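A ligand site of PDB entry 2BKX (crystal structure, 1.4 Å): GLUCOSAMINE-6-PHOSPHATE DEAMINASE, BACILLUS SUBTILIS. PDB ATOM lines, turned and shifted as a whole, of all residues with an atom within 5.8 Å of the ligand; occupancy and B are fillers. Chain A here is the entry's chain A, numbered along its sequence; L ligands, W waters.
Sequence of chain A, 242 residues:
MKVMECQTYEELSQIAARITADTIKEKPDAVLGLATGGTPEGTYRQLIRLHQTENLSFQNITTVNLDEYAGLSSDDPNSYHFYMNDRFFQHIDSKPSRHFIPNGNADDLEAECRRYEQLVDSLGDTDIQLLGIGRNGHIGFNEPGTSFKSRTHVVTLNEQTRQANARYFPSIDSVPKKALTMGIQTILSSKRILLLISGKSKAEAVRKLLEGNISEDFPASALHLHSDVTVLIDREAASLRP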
ATOM      1  N   LEU A  34     -14.572  20.034  31.802  1.00  0.00           N
ATOM      2  CA  LEU A  34     -13.179  19.679  32.028  1.00  0.00           C
ATOM      3  C   LEU A  34     -12.906  18.253  31.562  1.00  0.00           C
ATOM      4  O   LEU A  34     -13.816  17.449  31.409  1.00  0.00           O
ATOM      5  CB  LEU A  34     -12.827  19.860  33.515  1.00  0.00           C
ATOM      6  CG  LEU A  34     -12.935  21.313  33.999  1.00  0.00           C
ATOM      7  CD1 LEU A  34     -12.607  21.323  35.498  1.00  0.00           C
ATOM      8  CD2 LEU A  34     -12.021  22.265  33.253  1.00  0.00           C
ATOM      9  N   ALA A  35     -11.616  17.993  31.360  1.00  0.00           N
ATOM     10  CA  ALA A  35     -11.119  16.738  30.820  1.00  0.00           C
ATOM     11  C   ALA A  35      -9.993  16.183  31.679  1.00  0.00           C
ATOM     12  O   ALA A  35      -9.295  16.938  32.380  1.00  0.00           O
ATOM     13  CB  ALA A  35     -10.570  16.975  29.426  1.00  0.00           C
ATOM     14  N   THR A  36      -9.804  14.874  31.653  1.00  0.00           N
ATOM     15  CA  THR A  36      -8.683  14.221  32.300  1.00  0.00           C
ATOM     16  C   THR A  36      -7.700  13.734  31.238  1.00  0.00           C
ATOM     17  O   THR A  36      -7.735  14.197  30.088  1.00  0.00           O
ATOM     18  CB  THR A  36      -9.139  13.111  33.207  1.00  0.00           C
ATOM     19  OG1 THR A  36      -9.756  12.121  32.380  1.00  0.00           O
ATOM     20  CG2 THR A  36     -10.100  13.590  34.273  1.00  0.00           C
ATOM     21  N   GLY A  37      -6.820  12.823  31.632  1.00  0.00           N
ATOM     22  CA  GLY A  37      -5.776  12.330  30.738  1.00  0.00           C
ATOM     23  C   GLY A  37      -4.457  13.085  30.829  1.00  0.00           C
ATOM     24  O   GLY A  37      -4.272  14.001  31.616  1.00  0.00           O
ATOM     25  N   GLY A  38      -3.505  12.674  30.015  1.00  0.00           N
ATOM     26  CA  GLY A  38      -2.196  13.311  30.039  1.00  0.00           C
ATOM     27  C   GLY A  38      -2.227  14.714  29.454  1.00  0.00           C
ATOM     28  O   GLY A  38      -1.496  15.600  29.890  1.00  0.00           O
ATOM     29  N   THR A  39      -3.046  14.949  28.436  1.00  0.00           N
ATOM     30  CA  THR A  39      -2.919  16.194  27.717  1.00  0.00           C
ATOM     31  C   THR A  39      -3.131  17.464  28.560  1.00  0.00           C
ATOM     32  O   THR A  39      -2.353  18.386  28.433  1.00  0.00           O
ATOM     33  CB  THR A  39      -3.842  16.205  26.473  1.00  0.00           C
ATOM     34  OG1 THR A  39      -3.672  15.040  25.666  1.00  0.00           O
ATOM     35  CG2 THR A  39      -3.486  17.391  25.600  1.00  0.00           C
ATOM     36  N   PRO A  40      -4.188  17.521  29.397  1.00  0.00           N
ATOM     37  CA  PRO A  40      -4.423  18.751  30.159  1.00  0.00           C
ATOM     38  C   PRO A  40      -3.615  18.902  31.448  1.00  0.00           C
ATOM     39  O   PRO A  40      -3.819  19.865  32.186  1.00  0.00           O
ATOM     40  CB  PRO A  40      -5.915  18.704  30.452  1.00  0.00           C
ATOM     41  CG  PRO A  40      -6.183  17.255  30.618  1.00  0.00           C
ATOM     42  CD  PRO A  40      -5.297  16.556  29.589  1.00  0.00           C
ATOM     43  N   ASN A  65     -17.291  17.334  34.355  1.00  0.00           N
ATOM     44  CA  ASN A  65     -16.284  16.557  33.667  1.00  0.00           C
ATOM     45  C   ASN A  65     -16.907  15.691  32.562  1.00  0.00           C
ATOM     46  O   ASN A  65     -18.072  15.282  32.641  1.00  0.00           O
ATOM     47  CB  ASN A  65     -15.490  15.666  34.637  1.00  0.00           C
ATOM     48  CG  ASN A  65     -14.176  16.269  35.000  1.00  0.00           C
ATOM     49  OD1 ASN A  65     -13.089  15.809  34.504  1.00  0.00           O
ATOM     50  ND2 ASN A  65     -14.217  17.307  35.781  1.00  0.00           N
ATOM     51  N   LEU A  66     -16.104  15.408  31.556  1.00  0.00           N
ATOM     52  CA  LEU A  66     -16.541  14.599  30.416  1.00  0.00           C
ATOM     53  C   LEU A  66     -16.944  13.206  30.791  1.00  0.00           C
ATOM     54  O   LEU A  66     -17.905  12.652  30.229  1.00  0.00           O
ATOM     55  CB  LEU A  66     -15.418  14.508  29.370  1.00  0.00           C
ATOM     56  CG  LEU A  66     -15.139  15.749  28.552  1.00  0.00           C
ATOM     57  CD1 LEU A  66     -13.804  15.631  27.813  1.00  0.00           C
ATOM     58  CD2 LEU A  66     -16.236  15.984  27.550  1.00  0.00           C
ATOM     59  N   ASP A  67     -16.178  12.567  31.663  1.00  0.00           N
ATOM     60  CA  ASP A  67     -16.263  11.120  31.757  1.00  0.00           C
ATOM     61  C   ASP A  67     -15.762  10.543  33.058  1.00  0.00           C
ATOM     62  O   ASP A  67     -15.118  11.216  33.864  1.00  0.00           O
ATOM     63  CB  ASP A  67     -15.588  10.443  30.537  1.00  0.00           C
ATOM     64  CG  ASP A  67     -14.309  11.034  30.120  1.00  0.00           C
ATOM     65  OD1 ASP A  67     -14.151  11.011  28.878  1.00  0.00           O
ATOM     66  OD2 ASP A  67     -13.462  11.486  30.948  1.00  0.00           O
ATOM     67  N   TYR A  80     -11.452   9.156  37.597  1.00  0.00           N
ATOM     68  CA  TYR A  80     -11.341  10.543  37.203  1.00  0.00           C
ATOM     69  C   TYR A  80     -11.754  11.521  38.311  1.00  0.00           C
ATOM     70  O   TYR A  80     -11.293  12.679  38.316  1.00  0.00           O
ATOM     71  CB  TYR A  80     -12.069  10.762  35.877  1.00  0.00           C
ATOM     72  CG  TYR A  80     -11.337  10.090  34.699  1.00  0.00           C
ATOM     73  CD1 TYR A  80     -11.994   9.800  33.521  1.00  0.00           C
ATOM     74  CD2 TYR A  80      -9.986   9.777  34.762  1.00  0.00           C
ATOM     75  CE1 TYR A  80     -11.346   9.210  32.428  1.00  0.00           C
ATOM     76  CE2 TYR A  80      -9.337   9.187  33.686  1.00  0.00           C
ATOM     77  CZ  TYR A  80     -10.016   8.910  32.528  1.00  0.00           C
ATOM     78  OH  TYR A  80      -9.352   8.363  31.429  1.00  0.00           O
ATOM     79  N   LEU A 131     -11.326  19.639  25.840  1.00  0.00           N
ATOM     80  CA  LEU A 131     -11.318  18.309  25.277  1.00  0.00           C
ATOM     81  C   LEU A 131      -9.886  17.882  25.005  1.00  0.00           C
ATOM     82  O   LEU A 131      -9.011  18.709  24.750  1.00  0.00           O
ATOM     83  CB  LEU A 131     -12.017  18.274  23.909  1.00  0.00           C
ATOM     84  CG  LEU A 131     -13.453  18.609  23.853  1.00  0.00           C
ATOM     85  CD1 LEU A 131     -13.959  18.597  22.397  1.00  0.00           C
ATOM     86  CD2 LEU A 131     -14.294  17.652  24.709  1.00  0.00           C
ATOM     87  N   GLY A 132      -9.679  16.591  25.048  1.00  0.00           N
ATOM     88  CA  GLY A 132      -8.538  15.977  24.356  1.00  0.00           C
ATOM     89  C   GLY A 132      -9.056  15.162  23.175  1.00  0.00           C
ATOM     90  O   GLY A 132     -10.247  15.216  22.852  1.00  0.00           O
ATOM     91  N   ILE A 133      -8.170  14.427  22.516  1.00  0.00           N
ATOM     92  CA  ILE A 133      -8.546  13.596  21.370  1.00  0.00           C
ATOM     93  C   ILE A 133      -7.918  12.236  21.523  1.00  0.00           C
ATOM     94  O   ILE A 133      -6.749  12.125  21.863  1.00  0.00           O
ATOM     95  CB  ILE A 133      -8.165  14.256  20.023  1.00  0.00           C
ATOM     96  CG1 ILE A 133      -8.886  13.612  18.859  1.00  0.00           C
ATOM     97  CG2 ILE A 133      -6.667  14.301  19.799  1.00  0.00           C
ATOM     98  CD1 ILE A 133      -8.826  14.392  17.547  1.00  0.00           C
ATOM     99  N   GLY A 134      -8.693  11.203  21.252  1.00  0.00           N
ATOM    100  CA  GLY A 134      -8.131   9.884  21.243  1.00  0.00           C
ATOM    101  C   GLY A 134      -7.271   9.667  20.027  1.00  0.00           C
ATOM    102  O   GLY A 134      -7.398  10.373  19.004  1.00  0.00           O
ATOM    103  N   HIS A 138     -11.622   9.877  19.129  1.00  0.00           N
ATOM    104  CA  HIS A 138     -12.681  10.034  20.109  1.00  0.00           C
ATOM    105  C   HIS A 138     -12.592  11.364  20.822  1.00  0.00           C
ATOM    106  O   HIS A 138     -11.514  11.934  20.976  1.00  0.00           O
ATOM    107  CB  HIS A 138     -12.796   8.850  21.085  1.00  0.00           C
ATOM    108  CG  HIS A 138     -11.730   8.698  22.121  1.00  0.00           C
ATOM    109  ND1 HIS A 138     -11.205   7.460  22.414  1.00  0.00           N
ATOM    110  CD2 HIS A 138     -11.131   9.554  22.973  1.00  0.00           C
ATOM    111  CE1 HIS A 138     -10.323   7.566  23.400  1.00  0.00           C
ATOM    112  NE2 HIS A 138     -10.272   8.832  23.765  1.00  0.00           N
ATOM    113  N   ILE A 139     -13.731  11.840  21.270  1.00  0.00           N
ATOM    114  CA  ILE A 139     -13.862  12.987  22.166  1.00  0.00           C
ATOM    115  C   ILE A 139     -14.740  12.535  23.322  1.00  0.00           C
ATOM    116  O   ILE A 139     -15.672  11.783  23.132  1.00  0.00           O
ATOM    117  CB  ILE A 139     -14.350  14.283  21.484  1.00  0.00           C
ATOM    118  CG1 ILE A 139     -15.671  14.070  20.760  1.00  0.00           C
ATOM    119  CG2 ILE A 139     -13.276  14.797  20.530  1.00  0.00           C
ATOM    120  CD1 ILE A 139     -16.338  15.347  20.219  1.00  0.00           C
ATOM    121  N   GLY A 140     -14.409  12.939  24.524  1.00  0.00           N
ATOM    122  CA  GLY A 140     -14.857  12.195  25.688  1.00  0.00           C
ATOM    123  C   GLY A 140     -14.507  10.715  25.481  1.00  0.00           C
ATOM    124  O   GLY A 140     -13.432  10.419  24.975  1.00  0.00           O
ATOM    125  N   PHE A 141     -15.430   9.822  25.794  1.00  0.00           N
ATOM    126  CA  PHE A 141     -15.288   8.416  25.374  1.00  0.00           C
ATOM    127  C   PHE A 141     -16.320   8.038  24.314  1.00  0.00           C
ATOM    128  O   PHE A 141     -16.796   6.883  24.218  1.00  0.00           O
ATOM    129  CB  PHE A 141     -15.302   7.443  26.542  1.00  0.00           C
ATOM    130  CG  PHE A 141     -14.030   7.440  27.377  1.00  0.00           C
ATOM    131  CD1 PHE A 141     -14.155   7.316  28.732  1.00  0.00           C
ATOM    132  CD2 PHE A 141     -12.746   7.485  26.811  1.00  0.00           C
ATOM    133  CE1 PHE A 141     -13.007   7.201  29.555  1.00  0.00           C
ATOM    134  CE2 PHE A 141     -11.610   7.419  27.636  1.00  0.00           C
ATOM    135  CZ  PHE A 141     -11.748   7.260  28.991  1.00  0.00           C
ATOM    136  N   THR A 161      -8.376   2.405  23.039  1.00  0.00           N
ATOM    137  CA  THR A 161      -8.470   3.273  24.193  1.00  0.00           C
ATOM    138  C   THR A 161      -7.917   2.599  25.440  1.00  0.00           C
ATOM    139  O   THR A 161      -7.146   3.189  26.186  1.00  0.00           O
ATOM    140  CB  THR A 161      -9.911   3.668  24.401  1.00  0.00           C
ATOM    141  OG1 THR A 161     -10.333   4.346  23.226  1.00  0.00           O
ATOM    142  CG2 THR A 161     -10.075   4.562  25.614  1.00  0.00           C
ATOM    143  N   ASN A 165      -4.537   3.804  27.523  1.00  0.00           N
ATOM    144  CA  ASN A 165      -4.664   4.225  28.888  1.00  0.00           C
ATOM    145  C   ASN A 165      -4.035   3.221  29.854  1.00  0.00           C
ATOM    146  O   ASN A 165      -3.923   3.521  31.028  1.00  0.00           O
ATOM    147  CB  ASN A 165      -6.143   4.472  29.249  1.00  0.00           C
ATOM    148  CG  ASN A 165      -6.712   5.711  28.583  1.00  0.00           C
ATOM    149  OD1 ASN A 165      -6.031   6.307  27.743  1.00  0.00           O
ATOM    150  ND2 ASN A 165      -7.951   6.064  28.918  1.00  0.00           N
ATOM    151  N   ARG A 167      -1.062   2.569  30.446  1.00  0.00           N
ATOM    152  CA  ARG A 167       0.087   3.203  31.107  1.00  0.00           C
ATOM    153  C   ARG A 167      -0.220   3.723  32.484  1.00  0.00           C
ATOM    154  O   ARG A 167       0.666   3.864  33.308  1.00  0.00           O
ATOM    155  CB  ARG A 167       0.652   4.339  30.234  1.00  0.00           C
ATOM    156  CG  ARG A 167      -0.274   5.532  30.045  1.00  0.00           C
ATOM    157  CD  ARG A 167       0.065   6.410  28.739  1.00  0.00           C
ATOM    158  NE  ARG A 167      -0.466   7.814  28.737  1.00  0.00           N
ATOM    159  CZ  ARG A 167      -1.449   8.344  27.970  1.00  0.00           C
ATOM    160  NH1 ARG A 167      -2.076   7.627  27.016  1.00  0.00           N
ATOM    161  NH2 ARG A 167      -1.799   9.657  28.089  1.00  0.00           N
ATOM    162  N   TYR A 168      -1.493   4.001  32.755  1.00  0.00           N
ATOM    163  CA  TYR A 168      -1.870   4.524  34.074  1.00  0.00           C
ATOM    164  C   TYR A 168      -2.283   3.481  35.108  1.00  0.00           C
ATOM    165  O   TYR A 168      -2.521   3.847  36.265  1.00  0.00           O
ATOM    166  CB  TYR A 168      -3.014   5.514  33.871  1.00  0.00           C
ATOM    167  CG  TYR A 168      -2.579   6.726  33.063  1.00  0.00           C
ATOM    168  CD1 TYR A 168      -3.170   7.045  31.864  1.00  0.00           C
ATOM    169  CD2 TYR A 168      -1.487   7.491  33.456  1.00  0.00           C
ATOM    170  CE1 TYR A 168      -2.774   8.133  31.135  1.00  0.00           C
ATOM    171  CE2 TYR A 168      -1.074   8.593  32.738  1.00  0.00           C
ATOM    172  CZ  TYR A 168      -1.720   8.911  31.571  1.00  0.00           C
ATOM    173  OH  TYR A 168      -1.278   9.991  30.862  1.00  0.00           O
ATOM    174  N   THR A 181     -19.833   8.727  29.682  1.00  0.00           N
ATOM    175  CA  THR A 181     -19.307   9.905  28.993  1.00  0.00           C
ATOM    176  C   THR A 181     -20.437  10.833  28.549  1.00  0.00           C
ATOM    177  O   THR A 181     -21.494  10.402  28.115  1.00  0.00           O
ATOM    178  CB  THR A 181     -18.489   9.490  27.761  1.00  0.00           C
ATOM    179  OG1 THR A 181     -17.861  10.642  27.173  1.00  0.00           O
ATOM    180  CG2 THR A 181     -19.261   8.734  26.735  1.00  0.00           C
ATOM    181  N   SER A 201       1.763  10.542  19.222  1.00  0.00           N
ATOM    182  CA  SER A 201       0.682   9.579  19.191  1.00  0.00           C
ATOM    183  C   SER A 201      -0.611  10.096  18.610  1.00  0.00           C
ATOM    184  O   SER A 201      -1.447   9.287  18.237  1.00  0.00           O
ATOM    185  CB  SER A 201       0.416   9.009  20.586  1.00  0.00           C
ATOM    186  OG  SER A 201      -0.344   9.893  21.392  1.00  0.00           O
ATOM    187  N   LYS A 202      -0.753  11.430  18.541  1.00  0.00           N
ATOM    188  CA  LYS A 202      -1.948  12.064  18.015  1.00  0.00           C
ATOM    189  C   LYS A 202      -1.798  12.608  16.599  1.00  0.00           C
ATOM    190  O   LYS A 202      -2.736  13.221  16.052  1.00  0.00           O
ATOM    191  CB  LYS A 202      -2.374  13.219  18.939  1.00  0.00           C
ATOM    192  CG  LYS A 202      -2.525  12.808  20.401  1.00  0.00           C
ATOM    193  CD  LYS A 202      -3.497  11.651  20.609  1.00  0.00           C
ATOM    194  CE  LYS A 202      -3.649  11.288  22.096  1.00  0.00           C
ATOM    195  NZ  LYS A 202      -4.198  12.433  22.931  1.00  0.00           N
HETATM  196  C1  LIG L   1     -10.648  13.159  28.752  1.00  0.00           C
HETATM  197  C2  LIG L   1     -11.302  12.320  27.663  1.00  0.00           C
HETATM  198  C3  LIG L   1     -10.551  11.539  26.583  1.00  0.00           C
HETATM  199  C4  LIG L   1      -9.077  11.956  26.417  1.00  0.00           C
HETATM  200  C5  LIG L   1      -8.348  11.197  25.316  1.00  0.00           C
HETATM  201  C6  LIG L   1      -6.888  11.604  25.232  1.00  0.00           C
HETATM  202  O1  LIG L   1     -11.555  13.432  29.836  1.00  0.00           O
HETATM  203  O2  LIG L   1     -12.512  12.320  27.640  1.00  0.00           O
HETATM  204  O3  LIG L   1     -11.175  11.796  25.337  1.00  0.00           O
HETATM  205  O4  LIG L   1      -9.044  13.347  26.133  1.00  0.00           O
HETATM  206  O5  LIG L   1      -8.464   9.782  25.483  1.00  0.00           O
HETATM  207  O6  LIG L   1      -6.223  11.185  26.439  1.00  0.00           O
HETATM  208  P1  LIG L   1      -4.738  11.698  26.728  1.00  0.00           P
HETATM  209  O7  LIG L   1      -4.837  13.174  27.003  1.00  0.00           O
HETATM  210  O8  LIG L   1      -3.955  11.440  25.463  1.00  0.00           O
HETATM  211  O9  LIG L   1      -4.243  10.935  27.911  1.00  0.00           O
HETATM  212  O   HOH W   1      -8.442   8.919  28.177  1.00  0.00           O
HETATM  213  O   HOH W   2      -5.718   8.940  28.942  1.00  0.00           O
HETATM  214  O   HOH W   3     -10.391  10.512  29.642  1.00  0.00           O
HETATM  215  O   HOH W   4      -1.297  11.982  25.252  1.00  0.00           O
HETATM  216  O   HOH W   5      -6.537   7.779  25.285  1.00  0.00           O
HETATM  217  O   HOH W   6     -11.939  14.452  24.829  1.00  0.00           O
HETATM  218  O   HOH W   7      -3.817   8.784  24.970  1.00  0.00           O
HETATM  219  O   HOH W   8      -7.133  14.595  27.479  1.00  0.00           O
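An oxygen (O9) of the ligand is in salt-bridge range of the guanidinium group (NH2) of Arg 167 (2.8 Å).
The side-chain carboxylate of Asp 67 sits at hydrogen-bond distance from an oxygen (O1) of the ligand, at 2.9 Å.
A ring nitrogen (NE2) of His 138 lies within hydrogen-bond range of an oxygen (O5) of the ligand, at 2.7 Å.
N of Gly 132 sits close to O4 of the ligand (3.5 Å).
The backbone NH (N) of Thr 39 sits at hydrogen-bond distance from an oxygen (O7) of the ligand, 2.9 Å away.
The backbone NH (N) of Gly 38 is in hydrogen-bond range of an oxygen (O9) of the ligand (2.8 Å).
The backbone NH (N) of Thr 36 is in hydrogen-bond range of an oxygen (O1) of the ligand (2.9 Å).
An oxygen (O7) of the ligand sits at hydrogen-bond distance from the side-chain hydroxyl (OG1) of Thr 39 (2.6 Å).
An oxygen (O8) of the ligand is in salt-bridge range of the side-chain amino group (NZ) of Lys 202 (2.7 Å).
An oxygen (O1) of the ligand lies within hydrogen-bond range of the side-chain hydroxyl of Thr 36 (3.4 Å).
O of Gly 140 is in hydrogen-bond range of O3 of the ligand, at 2.7 Å.
ND1 of His 138 lies close to OG1 of Thr 161, 3.3 Å away.
NH2 of Arg 167 is in hydrogen-bond range of OH of Tyr 168.
O of Ile 133 is in hydrogen-bond range of NZ of Lys 202 (2.8 Å).
O of Leu 34 is in hydrogen-bond range of N of Leu 66 (3.1 Å).
Merely in contact with the ligand: Ala 35 (3.5 Å), Gly 37 (3.5 Å), Leu 66 (3.6 Å) and Ile 133 (3.4 Å).
Hydrophobic or aromatic side chains that line the ligand: Ala 35, Leu 66 and His 138.
Of the 26 residues printed, 13 come within 4 Å of the ligand.
The nearest printed residue that does not touch the ligand is Gly 134 (4.1 Å).
Water W8 lies within hydrogen-bond range of O4 of the ligand (2.6 Å) and O of Thr 36 (2.7 Å).
Water W7 lies within hydrogen-bond range of O8 of the ligand (2.7 Å) and NH1 of Arg 167 (2.9 Å).
Water W5 lies within hydrogen-bond range of O5 of the ligand and OD1 of Asn 165.
Water W3 lies within hydrogen-bond range of the side-chain hydroxyl (OH) of Tyr 80 (3.0 Å), an oxygen (O1) of the ligand (3.1 Å), the side-chain hydroxyl (OG1) of Thr 36 (3.2 Å) and the side-chain carboxylate (OD2) of Asp 67 (3.5 Å).
Water W6 lies within hydrogen-bond range of the backbone carbonyl oxygen (O) of Gly 132 (2.7 Å), an oxygen (O3) of the ligand (2.8 Å) and the backbone NH (N) of Gly 140 (2.9 Å).
Water W1 lies within hydrogen-bond range of an oxygen (O5) of the ligand (2.8 Å), the side-chain amide nitrogen of Asn 165 (3.0 Å) and the side-chain hydroxyl of Tyr 80 (3.4 Å).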
